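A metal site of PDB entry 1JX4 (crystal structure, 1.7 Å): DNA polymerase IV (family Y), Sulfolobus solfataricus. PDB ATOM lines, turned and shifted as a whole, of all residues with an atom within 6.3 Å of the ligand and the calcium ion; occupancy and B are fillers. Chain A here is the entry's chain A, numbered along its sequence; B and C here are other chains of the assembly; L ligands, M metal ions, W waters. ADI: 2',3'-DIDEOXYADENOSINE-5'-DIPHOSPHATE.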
ATOM      1  N   ASP A   7      -2.135  36.646 -17.927  1.00  0.00           N
ATOM      2  CA  ASP A   7      -2.459  35.238 -18.184  1.00  0.00           C
ATOM      3  C   ASP A   7      -1.331  34.442 -17.504  1.00  0.00           C
ATOM      4  O   ASP A   7      -0.173  34.528 -17.908  1.00  0.00           O
ATOM      5  CB  ASP A   7      -2.442  35.068 -19.703  1.00  0.00           C
ATOM      6  CG  ASP A   7      -2.722  33.633 -20.143  1.00  0.00           C
ATOM      7  OD1 ASP A   7      -2.353  32.638 -19.452  1.00  0.00           O
ATOM      8  OD2 ASP A   7      -3.320  33.541 -21.232  1.00  0.00           O
ATOM      9  N   PHE A   8      -1.658  33.724 -16.433  1.00  0.00           N
ATOM     10  CA  PHE A   8      -0.607  32.998 -15.710  1.00  0.00           C
ATOM     11  C   PHE A   8      -0.033  31.874 -16.581  1.00  0.00           C
ATOM     12  O   PHE A   8      -0.763  31.173 -17.293  1.00  0.00           O
ATOM     13  CB  PHE A   8      -1.129  32.395 -14.364  1.00  0.00           C
ATOM     14  CG  PHE A   8      -1.935  33.333 -13.480  1.00  0.00           C
ATOM     15  CD1 PHE A   8      -1.887  34.715 -13.656  1.00  0.00           C
ATOM     16  CD2 PHE A   8      -2.786  32.814 -12.464  1.00  0.00           C
ATOM     17  CE1 PHE A   8      -2.663  35.581 -12.869  1.00  0.00           C
ATOM     18  CE2 PHE A   8      -3.565  33.681 -11.663  1.00  0.00           C
ATOM     19  CZ  PHE A   8      -3.498  35.067 -11.886  1.00  0.00           C
ATOM     20  N   ASP A   9       1.281  31.664 -16.504  1.00  0.00           N
ATOM     21  CA  ASP A   9       1.867  30.639 -17.375  1.00  0.00           C
ATOM     22  C   ASP A   9       1.639  29.196 -16.912  1.00  0.00           C
ATOM     23  O   ASP A   9       1.831  28.876 -15.732  1.00  0.00           O
ATOM     24  CB  ASP A   9       3.373  30.909 -17.556  1.00  0.00           C
ATOM     25  CG  ASP A   9       3.679  32.331 -18.117  1.00  0.00           C
ATOM     26  OD1 ASP A   9       2.932  32.781 -19.019  1.00  0.00           O
ATOM     27  OD2 ASP A   9       4.668  32.963 -17.693  1.00  0.00           O
ATOM     28  N   TYR A  10       1.267  28.328 -17.852  1.00  0.00           N
ATOM     29  CA  TYR A  10       1.004  26.912 -17.602  1.00  0.00           C
ATOM     30  C   TYR A  10       0.612  26.717 -16.150  1.00  0.00           C
ATOM     31  O   TYR A  10       1.105  25.831 -15.421  1.00  0.00           O
ATOM     32  CB  TYR A  10       2.266  26.048 -17.962  1.00  0.00           C
ATOM     33  CG  TYR A  10       3.567  26.411 -17.295  1.00  0.00           C
ATOM     34  CD1 TYR A  10       4.109  25.602 -16.258  1.00  0.00           C
ATOM     35  CD2 TYR A  10       4.298  27.548 -17.697  1.00  0.00           C
ATOM     36  CE1 TYR A  10       5.367  25.932 -15.626  1.00  0.00           C
ATOM     37  CE2 TYR A  10       5.542  27.892 -17.055  1.00  0.00           C
ATOM     38  CZ  TYR A  10       6.052  27.069 -16.023  1.00  0.00           C
ATOM     39  OH  TYR A  10       7.192  27.478 -15.322  1.00  0.00           O
ATOM     40  N   PHE A  11      -0.395  27.489 -15.758  1.00  0.00           N
ATOM     41  CA  PHE A  11      -0.696  27.590 -14.350  1.00  0.00           C
ATOM     42  C   PHE A  11      -0.657  26.422 -13.393  1.00  0.00           C
ATOM     43  O   PHE A  11       0.106  26.493 -12.434  1.00  0.00           O
ATOM     44  CB  PHE A  11      -2.009  28.406 -14.164  1.00  0.00           C
ATOM     45  CG  PHE A  11      -2.255  28.854 -12.727  1.00  0.00           C
ATOM     46  CD1 PHE A  11      -1.284  29.595 -12.033  1.00  0.00           C
ATOM     47  CD2 PHE A  11      -3.430  28.540 -12.058  1.00  0.00           C
ATOM     48  CE1 PHE A  11      -1.473  30.008 -10.682  1.00  0.00           C
ATOM     49  CE2 PHE A  11      -3.643  28.947 -10.704  1.00  0.00           C
ATOM     50  CZ  PHE A  11      -2.645  29.692 -10.028  1.00  0.00           C
ATOM     51  N   TYR A  12      -1.446  25.350 -13.589  1.00  0.00           N
ATOM     52  CA  TYR A  12      -1.466  24.298 -12.597  1.00  0.00           C
ATOM     53  C   TYR A  12      -0.084  23.626 -12.470  1.00  0.00           C
ATOM     54  O   TYR A  12       0.376  23.278 -11.355  1.00  0.00           O
ATOM     55  CB  TYR A  12      -2.479  23.235 -12.935  1.00  0.00           C
ATOM     56  CG  TYR A  12      -3.906  23.701 -13.074  1.00  0.00           C
ATOM     57  CD1 TYR A  12      -4.332  24.949 -12.582  1.00  0.00           C
ATOM     58  CD2 TYR A  12      -4.849  22.878 -13.637  1.00  0.00           C
ATOM     59  CE1 TYR A  12      -5.681  25.319 -12.659  1.00  0.00           C
ATOM     60  CE2 TYR A  12      -6.201  23.241 -13.678  1.00  0.00           C
ATOM     61  CZ  TYR A  12      -6.581  24.448 -13.195  1.00  0.00           C
ATOM     62  OH  TYR A  12      -7.911  24.775 -13.265  1.00  0.00           O
ATOM     63  N   ALA A  13       0.562  23.445 -13.616  1.00  0.00           N
ATOM     64  CA  ALA A  13       1.875  22.815 -13.573  1.00  0.00           C
ATOM     65  C   ALA A  13       2.852  23.757 -12.926  1.00  0.00           C
ATOM     66  O   ALA A  13       3.720  23.284 -12.186  1.00  0.00           O
ATOM     67  CB  ALA A  13       2.339  22.424 -14.978  1.00  0.00           C
ATOM     68  N   VAL A  32      -6.248  14.740 -14.961  1.00  0.00           N
ATOM     69  CA  VAL A  32      -7.566  14.543 -14.370  1.00  0.00           C
ATOM     70  C   VAL A  32      -7.810  13.050 -14.566  1.00  0.00           C
ATOM     71  O   VAL A  32      -8.157  12.609 -15.664  1.00  0.00           O
ATOM     72  CB  VAL A  32      -8.618  15.411 -15.128  1.00  0.00           C
ATOM     73  CG1 VAL A  32      -9.932  15.343 -14.410  1.00  0.00           C
ATOM     74  CG2 VAL A  32      -8.141  16.871 -15.236  1.00  0.00           C
ATOM     75  N   VAL A  43      -5.287  15.041 -19.764  1.00  0.00           N
ATOM     76  CA  VAL A  43      -4.330  16.030 -19.278  1.00  0.00           C
ATOM     77  C   VAL A  43      -4.992  17.416 -19.088  1.00  0.00           C
ATOM     78  O   VAL A  43      -5.701  17.928 -20.009  1.00  0.00           O
ATOM     79  CB  VAL A  43      -3.155  16.184 -20.316  1.00  0.00           C
ATOM     80  CG1 VAL A  43      -2.218  17.369 -19.896  1.00  0.00           C
ATOM     81  CG2 VAL A  43      -2.444  14.826 -20.368  1.00  0.00           C
ATOM     82  N   ALA A  44      -4.833  18.013 -17.906  1.00  0.00           N
ATOM     83  CA  ALA A  44      -5.413  19.362 -17.688  1.00  0.00           C
ATOM     84  C   ALA A  44      -4.498  20.393 -18.216  1.00  0.00           C
ATOM     85  O   ALA A  44      -4.945  21.410 -18.774  1.00  0.00           O
ATOM     86  CB  ALA A  44      -5.648  19.636 -16.225  1.00  0.00           C
ATOM     87  N   THR A  45      -3.199  20.195 -17.962  1.00  0.00           N
ATOM     88  CA  THR A  45      -2.206  21.096 -18.490  1.00  0.00           C
ATOM     89  C   THR A  45      -0.826  20.490 -18.298  1.00  0.00           C
ATOM     90  O   THR A  45      -0.590  19.624 -17.428  1.00  0.00           O
ATOM     91  CB  THR A  45      -2.246  22.486 -17.851  1.00  0.00           C
ATOM     92  OG1 THR A  45      -1.351  23.359 -18.557  1.00  0.00           O
ATOM     93  CG2 THR A  45      -1.793  22.409 -16.436  1.00  0.00           C
ATOM     94  N   ALA A  46       0.116  20.939 -19.092  1.00  0.00           N
ATOM     95  CA  ALA A  46       1.465  20.429 -18.944  1.00  0.00           C
ATOM     96  C   ALA A  46       2.364  21.659 -19.029  1.00  0.00           C
ATOM     97  O   ALA A  46       1.949  22.679 -19.595  1.00  0.00           O
ATOM     98  CB  ALA A  46       1.774  19.471 -20.060  1.00  0.00           C
ATOM     99  N   TYR A  48       5.905  23.793 -20.270  1.00  0.00           N
ATOM    100  CA  TYR A  48       6.395  23.860 -21.617  1.00  0.00           C
ATOM    101  C   TYR A  48       7.373  22.757 -22.007  1.00  0.00           C
ATOM    102  O   TYR A  48       7.440  22.431 -23.167  1.00  0.00           O
ATOM    103  CB  TYR A  48       6.939  25.256 -21.915  1.00  0.00           C
ATOM    104  CG  TYR A  48       5.785  26.264 -22.134  1.00  0.00           C
ATOM    105  CD1 TYR A  48       5.027  26.730 -21.059  1.00  0.00           C
ATOM    106  CD2 TYR A  48       5.453  26.720 -23.428  1.00  0.00           C
ATOM    107  CE1 TYR A  48       3.981  27.605 -21.251  1.00  0.00           C
ATOM    108  CE2 TYR A  48       4.394  27.627 -23.632  1.00  0.00           C
ATOM    109  CZ  TYR A  48       3.670  28.067 -22.534  1.00  0.00           C
ATOM    110  OH  TYR A  48       2.621  28.982 -22.744  1.00  0.00           O
ATOM    111  N   ARG A  51       4.981  20.235 -23.362  1.00  0.00           N
ATOM    112  CA  ARG A  51       4.327  20.659 -24.597  1.00  0.00           C
ATOM    113  C   ARG A  51       5.209  20.609 -25.823  1.00  0.00           C
ATOM    114  O   ARG A  51       4.702  20.324 -26.925  1.00  0.00           O
ATOM    115  CB  ARG A  51       3.810  22.091 -24.519  1.00  0.00           C
ATOM    116  CG  ARG A  51       2.907  22.345 -23.382  1.00  0.00           C
ATOM    117  CD  ARG A  51       2.335  23.779 -23.482  1.00  0.00           C
ATOM    118  NE  ARG A  51       1.677  24.040 -22.215  1.00  0.00           N
ATOM    119  CZ  ARG A  51       0.936  25.099 -21.932  1.00  0.00           C
ATOM    120  NH1 ARG A  51       0.715  26.062 -22.850  1.00  0.00           N
ATOM    121  NH2 ARG A  51       0.440  25.191 -20.709  1.00  0.00           N
ATOM    122  N   ALA A  57      -2.855  20.068 -22.861  1.00  0.00           N
ATOM    123  CA  ALA A  57      -4.206  19.978 -22.324  1.00  0.00           C
ATOM    124  C   ALA A  57      -5.145  19.258 -23.273  1.00  0.00           C
ATOM    125  O   ALA A  57      -5.163  19.550 -24.494  1.00  0.00           O
ATOM    126  CB  ALA A  57      -4.760  21.396 -22.034  1.00  0.00           C
ATOM    127  N   GLY A  58      -5.896  18.306 -22.747  1.00  0.00           N
ATOM    128  CA  GLY A  58      -6.916  17.672 -23.555  1.00  0.00           C
ATOM    129  C   GLY A  58      -6.698  16.242 -24.037  1.00  0.00           C
ATOM    130  O   GLY A  58      -7.633  15.536 -24.276  1.00  0.00           O
ATOM    131  N   MET A  76      -4.540  16.572 -10.552  1.00  0.00           N
ATOM    132  CA  MET A  76      -4.969  17.996 -10.447  1.00  0.00           C
ATOM    133  C   MET A  76      -5.382  18.258  -8.955  1.00  0.00           C
ATOM    134  O   MET A  76      -6.117  17.456  -8.403  1.00  0.00           O
ATOM    135  CB  MET A  76      -6.181  18.185 -11.349  1.00  0.00           C
ATOM    136  CG  MET A  76      -6.232  19.461 -12.254  1.00  0.00           C
ATOM    137  SD  MET A  76      -8.073  19.988 -12.696  1.00  0.00           S
ATOM    138  CE  MET A  76      -7.758  20.820 -14.426  1.00  0.00           C
ATOM    139  N   SER A 103     -11.133  33.860 -15.476  1.00  0.00           N
ATOM    140  CA  SER A 103     -11.052  32.448 -15.147  1.00  0.00           C
ATOM    141  C   SER A 103     -10.042  32.292 -14.008  1.00  0.00           C
ATOM    142  O   SER A 103      -9.544  33.288 -13.480  1.00  0.00           O
ATOM    143  CB  SER A 103     -10.569  31.664 -16.359  1.00  0.00           C
ATOM    144  OG  SER A 103      -9.209  31.990 -16.634  1.00  0.00           O
ATOM    145  N   ILE A 104      -9.697  31.060 -13.676  1.00  0.00           N
ATOM    146  CA  ILE A 104      -8.751  30.854 -12.596  1.00  0.00           C
ATOM    147  C   ILE A 104      -7.381  31.461 -12.924  1.00  0.00           C
ATOM    148  O   ILE A 104      -6.597  31.711 -11.999  1.00  0.00           O
ATOM    149  CB  ILE A 104      -8.625  29.340 -12.255  1.00  0.00           C
ATOM    150  CG1 ILE A 104      -7.943  29.162 -10.899  1.00  0.00           C
ATOM    151  CG2 ILE A 104      -8.015  28.603 -13.438  1.00  0.00           C
ATOM    152  CD1 ILE A 104      -8.045  27.736 -10.360  1.00  0.00           C
ATOM    153  N   ASP A 105      -7.058  31.730 -14.208  1.00  0.00           N
ATOM    154  CA  ASP A 105      -5.732  32.302 -14.405  1.00  0.00           C
ATOM    155  C   ASP A 105      -5.654  33.454 -15.402  1.00  0.00           C
ATOM    156  O   ASP A 105      -4.609  33.729 -15.992  1.00  0.00           O
ATOM    157  CB  ASP A 105      -4.716  31.215 -14.722  1.00  0.00           C
ATOM    158  CG  ASP A 105      -4.714  30.814 -16.215  1.00  0.00           C
ATOM    159  OD1 ASP A 105      -5.800  30.839 -16.808  1.00  0.00           O
ATOM    160  OD2 ASP A 105      -3.613  30.477 -16.737  1.00  0.00           O
ATOM    161  N   GLU A 106      -6.773  34.130 -15.575  1.00  0.00           N
ATOM    162  CA  GLU A 106      -6.767  35.271 -16.492  1.00  0.00           C
ATOM    163  C   GLU A 106      -7.534  36.431 -15.911  1.00  0.00           C
ATOM    164  O   GLU A 106      -8.619  36.236 -15.337  1.00  0.00           O
ATOM    165  CB  GLU A 106      -7.489  34.899 -17.762  1.00  0.00           C
ATOM    166  CG  GLU A 106      -7.005  33.728 -18.510  1.00  0.00           C
ATOM    167  CD  GLU A 106      -8.022  33.459 -19.597  1.00  0.00           C
ATOM    168  OE1 GLU A 106      -9.156  33.140 -19.239  1.00  0.00           O
ATOM    169  OE2 GLU A 106      -7.755  33.601 -20.773  1.00  0.00           O
ATOM    170  N   LYS A 159       3.330  34.567 -24.730  1.00  0.00           N
ATOM    171  CA  LYS A 159       3.530  33.565 -23.659  1.00  0.00           C
ATOM    172  C   LYS A 159       4.552  32.503 -24.073  1.00  0.00           C
ATOM    173  O   LYS A 159       4.699  32.209 -25.269  1.00  0.00           O
ATOM    174  CB  LYS A 159       2.199  32.902 -23.253  1.00  0.00           C
ATOM    175  CG  LYS A 159       1.533  32.097 -24.370  1.00  0.00           C
ATOM    176  CD  LYS A 159       0.238  31.389 -23.872  1.00  0.00           C
ATOM    177  CE  LYS A 159      -0.727  32.332 -23.160  1.00  0.00           C
ATOM    178  NZ  LYS A 159      -2.112  31.763 -22.926  1.00  0.00           N
ATOM    179  P    DT B   5     -13.533  12.337 -20.805  1.00  0.00           P
ATOM    180  OP1  DT B   5     -13.944  10.992 -20.360  1.00  0.00           O
ATOM    181  OP2  DT B   5     -14.547  13.243 -21.464  1.00  0.00           O
ATOM    182  O5'  DT B   5     -12.880  13.029 -19.535  1.00  0.00           O
ATOM    183  C5'  DT B   5     -11.996  12.303 -18.696  1.00  0.00           C
ATOM    184  C4'  DT B   5     -11.744  13.109 -17.448  1.00  0.00           C
ATOM    185  O4'  DT B   5     -10.942  14.253 -17.800  1.00  0.00           O
ATOM    186  C3'  DT B   5     -13.031  13.662 -16.862  1.00  0.00           C
ATOM    187  O3'  DT B   5     -12.876  13.678 -15.453  1.00  0.00           O
ATOM    188  C2'  DT B   5     -13.120  15.074 -17.446  1.00  0.00           C
ATOM    189  C1'  DT B   5     -11.647  15.473 -17.632  1.00  0.00           C
ATOM    190  N1   DT B   5     -11.315  16.296 -18.828  1.00  0.00           N
ATOM    191  C2   DT B   5     -10.770  17.562 -18.628  1.00  0.00           C
ATOM    192  O2   DT B   5     -10.586  18.047 -17.554  1.00  0.00           O
ATOM    193  N3   DT B   5     -10.424  18.211 -19.777  1.00  0.00           N
ATOM    194  C4   DT B   5     -10.539  17.764 -21.058  1.00  0.00           C
ATOM    195  O4   DT B   5     -10.123  18.449 -21.999  1.00  0.00           O
ATOM    196  C5   DT B   5     -11.144  16.471 -21.210  1.00  0.00           C
ATOM    197  C7   DT B   5     -11.321  15.960 -22.600  1.00  0.00           C
ATOM    198  C6   DT B   5     -11.502  15.803 -20.091  1.00  0.00           C
ATOM    199  P    DT B   6     -14.165  13.972 -14.531  1.00  0.00           P
ATOM    200  OP1  DT B   6     -13.812  13.431 -13.210  1.00  0.00           O
ATOM    201  OP2  DT B   6     -15.334  13.485 -15.268  1.00  0.00           O
ATOM    202  O5'  DT B   6     -14.231  15.555 -14.452  1.00  0.00           O
ATOM    203  C5'  DT B   6     -13.274  16.220 -13.697  1.00  0.00           C
ATOM    204  C4'  DT B   6     -13.380  17.704 -13.921  1.00  0.00           C
ATOM    205  O4'  DT B   6     -13.069  17.980 -15.304  1.00  0.00           O
ATOM    206  C3'  DT B   6     -14.758  18.353 -13.661  1.00  0.00           C
ATOM    207  O3'  DT B   6     -14.624  19.168 -12.504  1.00  0.00           O
ATOM    208  C2'  DT B   6     -15.021  19.195 -14.918  1.00  0.00           C
ATOM    209  C1'  DT B   6     -13.617  19.268 -15.574  1.00  0.00           C
ATOM    210  N1   DT B   6     -13.592  19.457 -17.044  1.00  0.00           N
ATOM    211  C2   DT B   6     -12.935  20.585 -17.519  1.00  0.00           C
ATOM    212  O2   DT B   6     -12.438  21.407 -16.780  1.00  0.00           O
ATOM    213  N3   DT B   6     -12.867  20.668 -18.883  1.00  0.00           N
ATOM    214  C4   DT B   6     -13.374  19.778 -19.799  1.00  0.00           C
ATOM    215  O4   DT B   6     -13.181  19.946 -20.986  1.00  0.00           O
ATOM    216  C5   DT B   6     -14.100  18.648 -19.245  1.00  0.00           C
ATOM    217  C7   DT B   6     -14.763  17.678 -20.164  1.00  0.00           C
ATOM    218  C6   DT B   6     -14.160  18.552 -17.899  1.00  0.00           C
ATOM    219  P    DA C  13      -8.925  30.532 -23.919  1.00  0.00           P
ATOM    220  OP1  DA C  13      -8.130  31.791 -24.043  1.00  0.00           O
ATOM    221  OP2  DA C  13      -8.631  29.392 -24.840  1.00  0.00           O
ATOM    222  O5'  DA C  13      -8.809  30.060 -22.407  1.00  0.00           O
ATOM    223  C5'  DA C  13      -9.474  30.802 -21.367  1.00  0.00           C
ATOM    224  C4'  DA C  13      -9.396  30.041 -20.069  1.00  0.00           C
ATOM    225  O4'  DA C  13     -10.234  28.852 -20.149  1.00  0.00           O
ATOM    226  C3'  DA C  13      -7.982  29.545 -19.771  1.00  0.00           C
ATOM    227  C2'  DA C  13      -8.015  28.106 -20.261  1.00  0.00           C
ATOM    228  C1'  DA C  13      -9.448  27.697 -19.899  1.00  0.00           C
ATOM    229  N9   DA C  13      -9.973  26.572 -20.681  1.00  0.00           N
ATOM    230  C8   DA C  13      -9.866  26.393 -22.021  1.00  0.00           C
ATOM    231  N7   DA C  13     -10.331  25.242 -22.439  1.00  0.00           N
ATOM    232  C5   DA C  13     -10.822  24.644 -21.290  1.00  0.00           C
ATOM    233  C6   DA C  13     -11.399  23.385 -21.055  1.00  0.00           C
ATOM    234  N6   DA C  13     -11.579  22.466 -22.001  1.00  0.00           N
ATOM    235  N1   DA C  13     -11.766  23.094 -19.792  1.00  0.00           N
ATOM    236  C2   DA C  13     -11.508  23.977 -18.826  1.00  0.00           C
ATOM    237  N3   DA C  13     -10.940  25.173 -18.919  1.00  0.00           N
ATOM    238  C4   DA C  13     -10.622  25.453 -20.199  1.00  0.00           C
HETATM  239  PB  ADI L   1      -2.215  28.388 -21.481  1.00  0.00           P
HETATM  240  O1B ADI L   1      -2.212  29.761 -20.788  1.00  0.00           O
HETATM  241  O2B ADI L   1      -2.909  28.195 -22.755  1.00  0.00           O
HETATM  242  O3B ADI L   1      -0.725  28.037 -21.456  1.00  0.00           O
HETATM  243  PA  ADI L   1      -2.683  27.109 -18.886  1.00  0.00           P
HETATM  244  O1A ADI L   1      -2.100  28.398 -18.281  1.00  0.00           O
HETATM  245  O2A ADI L   1      -1.960  25.827 -18.797  1.00  0.00           O
HETATM  246  O3A ADI L   1      -3.040  27.571 -20.389  1.00  0.00           O
HETATM  247  O5' ADI L   1      -4.198  26.866 -18.411  1.00  0.00           O
HETATM  248  C5' ADI L   1      -4.859  27.608 -17.363  1.00  0.00           C
HETATM  249  C4' ADI L   1      -5.709  26.618 -16.565  1.00  0.00           C
HETATM  250  O4' ADI L   1      -6.704  26.327 -17.573  1.00  0.00           O
HETATM  251  C3' ADI L   1      -4.866  25.358 -16.337  1.00  0.00           C
HETATM  252  C2' ADI L   1      -5.980  24.361 -16.594  1.00  0.00           C
HETATM  253  C1' ADI L   1      -7.034  24.958 -17.479  1.00  0.00           C
HETATM  254  N9  ADI L   1      -7.237  24.183 -18.719  1.00  0.00           N
HETATM  255  C8  ADI L   1      -6.835  24.485 -20.027  1.00  0.00           C
HETATM  256  N7  ADI L   1      -7.247  23.609 -20.895  1.00  0.00           N
HETATM  257  C5  ADI L   1      -7.910  22.659 -20.141  1.00  0.00           C
HETATM  258  C6  ADI L   1      -8.561  21.439 -20.483  1.00  0.00           C
HETATM  259  N6  ADI L   1      -8.606  20.948 -21.717  1.00  0.00           N
HETATM  260  N1  ADI L   1      -9.149  20.743 -19.447  1.00  0.00           N
HETATM  261  C2  ADI L   1      -9.085  21.191 -18.169  1.00  0.00           C
HETATM  262  N3  ADI L   1      -8.483  22.283 -17.723  1.00  0.00           N
HETATM  263  C4  ADI L   1      -7.916  22.982 -18.794  1.00  0.00           C
HETATM  264 CA    CA M   1      -2.493  30.568 -18.658  1.00  0.00          CA
HETATM  265  O   HOH W   1      -6.451  24.774 -23.151  1.00  0.00           O
HETATM  266  O   HOH W   2      -4.929  30.668 -19.518  1.00  0.00           O
HETATM  267  O   HOH W   3      -7.629  22.632 -24.091  1.00  0.00           O
HETATM  268  O   HOH W   4       1.112  29.362 -20.585  1.00  0.00           O
HETATM  269  O   HOH W   5      -3.978  25.546 -22.929  1.00  0.00           O
HETATM  270  O   HOH W   6      -1.449  27.972 -25.047  1.00  0.00           O
HETATM  271  O   HOH W   7      -9.377  23.017 -15.106  1.00  0.00           O
HETATM  272  O   HOH W   8      -4.863  30.088 -22.940  1.00  0.00           O
HETATM  273  O   HOH W   9      -3.251  23.969 -20.484  1.00  0.00           O
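Of the 25 residues printed, 3 come within 4 Å of the calcium ion.
Water W4 lies within hydrogen-bond range of an oxygen (O3B) of the ligand (2.4 Å), the side-chain hydroxyl of Tyr 48 (2.7 Å) and the backbone NH of Tyr 10 (2.9 Å). Water W8 lies within hydrogen-bond range of O2B of the ligand and NZ of Lys 159. Water W9 lies within hydrogen-bond range of the side-chain hydroxyl of Thr 45 (2.8 Å) and an oxygen (O2A) of the ligand (2.8 Å). Water W7 bridges N3 of the ligand (2.9 Å) and OH of Tyr 12 (2.9 Å).
OD1 of Asp 7 binds the calcium ion, 2.2 Å away. The side-chain carboxylate (OD2) of Asp 105 is bound to the calcium ion (2.2 Å). O1A of the ligand is bound to the calcium ion (2.2 Å). The calcium ion is bound by the backbone carbonyl oxygen (O) of Phe 8 (2.3 Å). O1B of the ligand is bound to the calcium ion (2.3 Å). The calcium ion is bound by water W2, 2.6 Å away. The calcium ion has six donor atoms within binding distance.
The side-chain carboxylate of Asp 7 is in salt-bridge range of the side-chain amino group of Lys 159. N of Asp 105 sits close to OG of Ser 103 (3.3 Å). The side-chain hydroxyl (OG1) of Thr 45 lies within hydrogen-bond range of the guanidinium group (NH2) of Arg 51 (3.3 Å). OH of Tyr 48 sits at hydrogen-bond distance from NH1 of Arg 51, 3.5 Å away. NE of Arg 51 sits at hydrogen-bond distance from O of Ala 46 (3.0 Å). O of Val 43 is in hydrogen-bond range of N of Gly 58, 2.8 Å away.
An oxygen (O2A) of the ligand sits at hydrogen-bond distance from the side-chain hydroxyl (OG1) of Thr 45 (2.6 Å). The guanidinium group (NH1) of Arg 51 is in salt-bridge range of an oxygen (O3B) of the ligand (2.8 Å). A nitrogen (N6) of the ligand is in hydrogen-bond range of O4 of DT 5 of chain B (2.9 Å). An oxygen (O2B) of the ligand is in salt-bridge range of the side-chain amino group of Lys 159 (3.7 Å). The backbone NH (N) of Phe 11 sits close to an oxygen (O1A) of the ligand (3.2 Å). N6 of DA 13 of chain C lies within hydrogen-bond range of N6 of the ligand (3.4 Å). O1A of the ligand lies close to N of Tyr 10 (3.4 Å).
CE2 of Tyr 12 touches C2' of the ligand, at 3.1 Å. Ala 44 touches the ligand. Tyr 48 touches the ligand. Ala 57 touches the ligand (CB to N7, 3.5 Å). Gly 58 touches the ligand (N to N6, 3.9 Å). Met 76 touches the ligand (CE to N3, 3.7 Å). DT 6 of chain B touches the ligand (O2 to C2, 3.6 Å). Hydrophobic or aromatic side chains that line the ligand: Tyr 12, Ala 57 and Met 76. 17 residues have an atom within 4 Å of the ligand: Asp 7, Phe 8, Tyr 10, Phe 11, Tyr 12, Ala 44, Thr 45, Tyr 48, Arg 51, Ala 57, Gly 58, Met 76, Asp 105, Lys 159, DT 5 of chain B, DT 6 of chain B and DA 13 of chain C. The nearest printed residue that does not touch the ligand is Asp 9 (4.1 Å).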
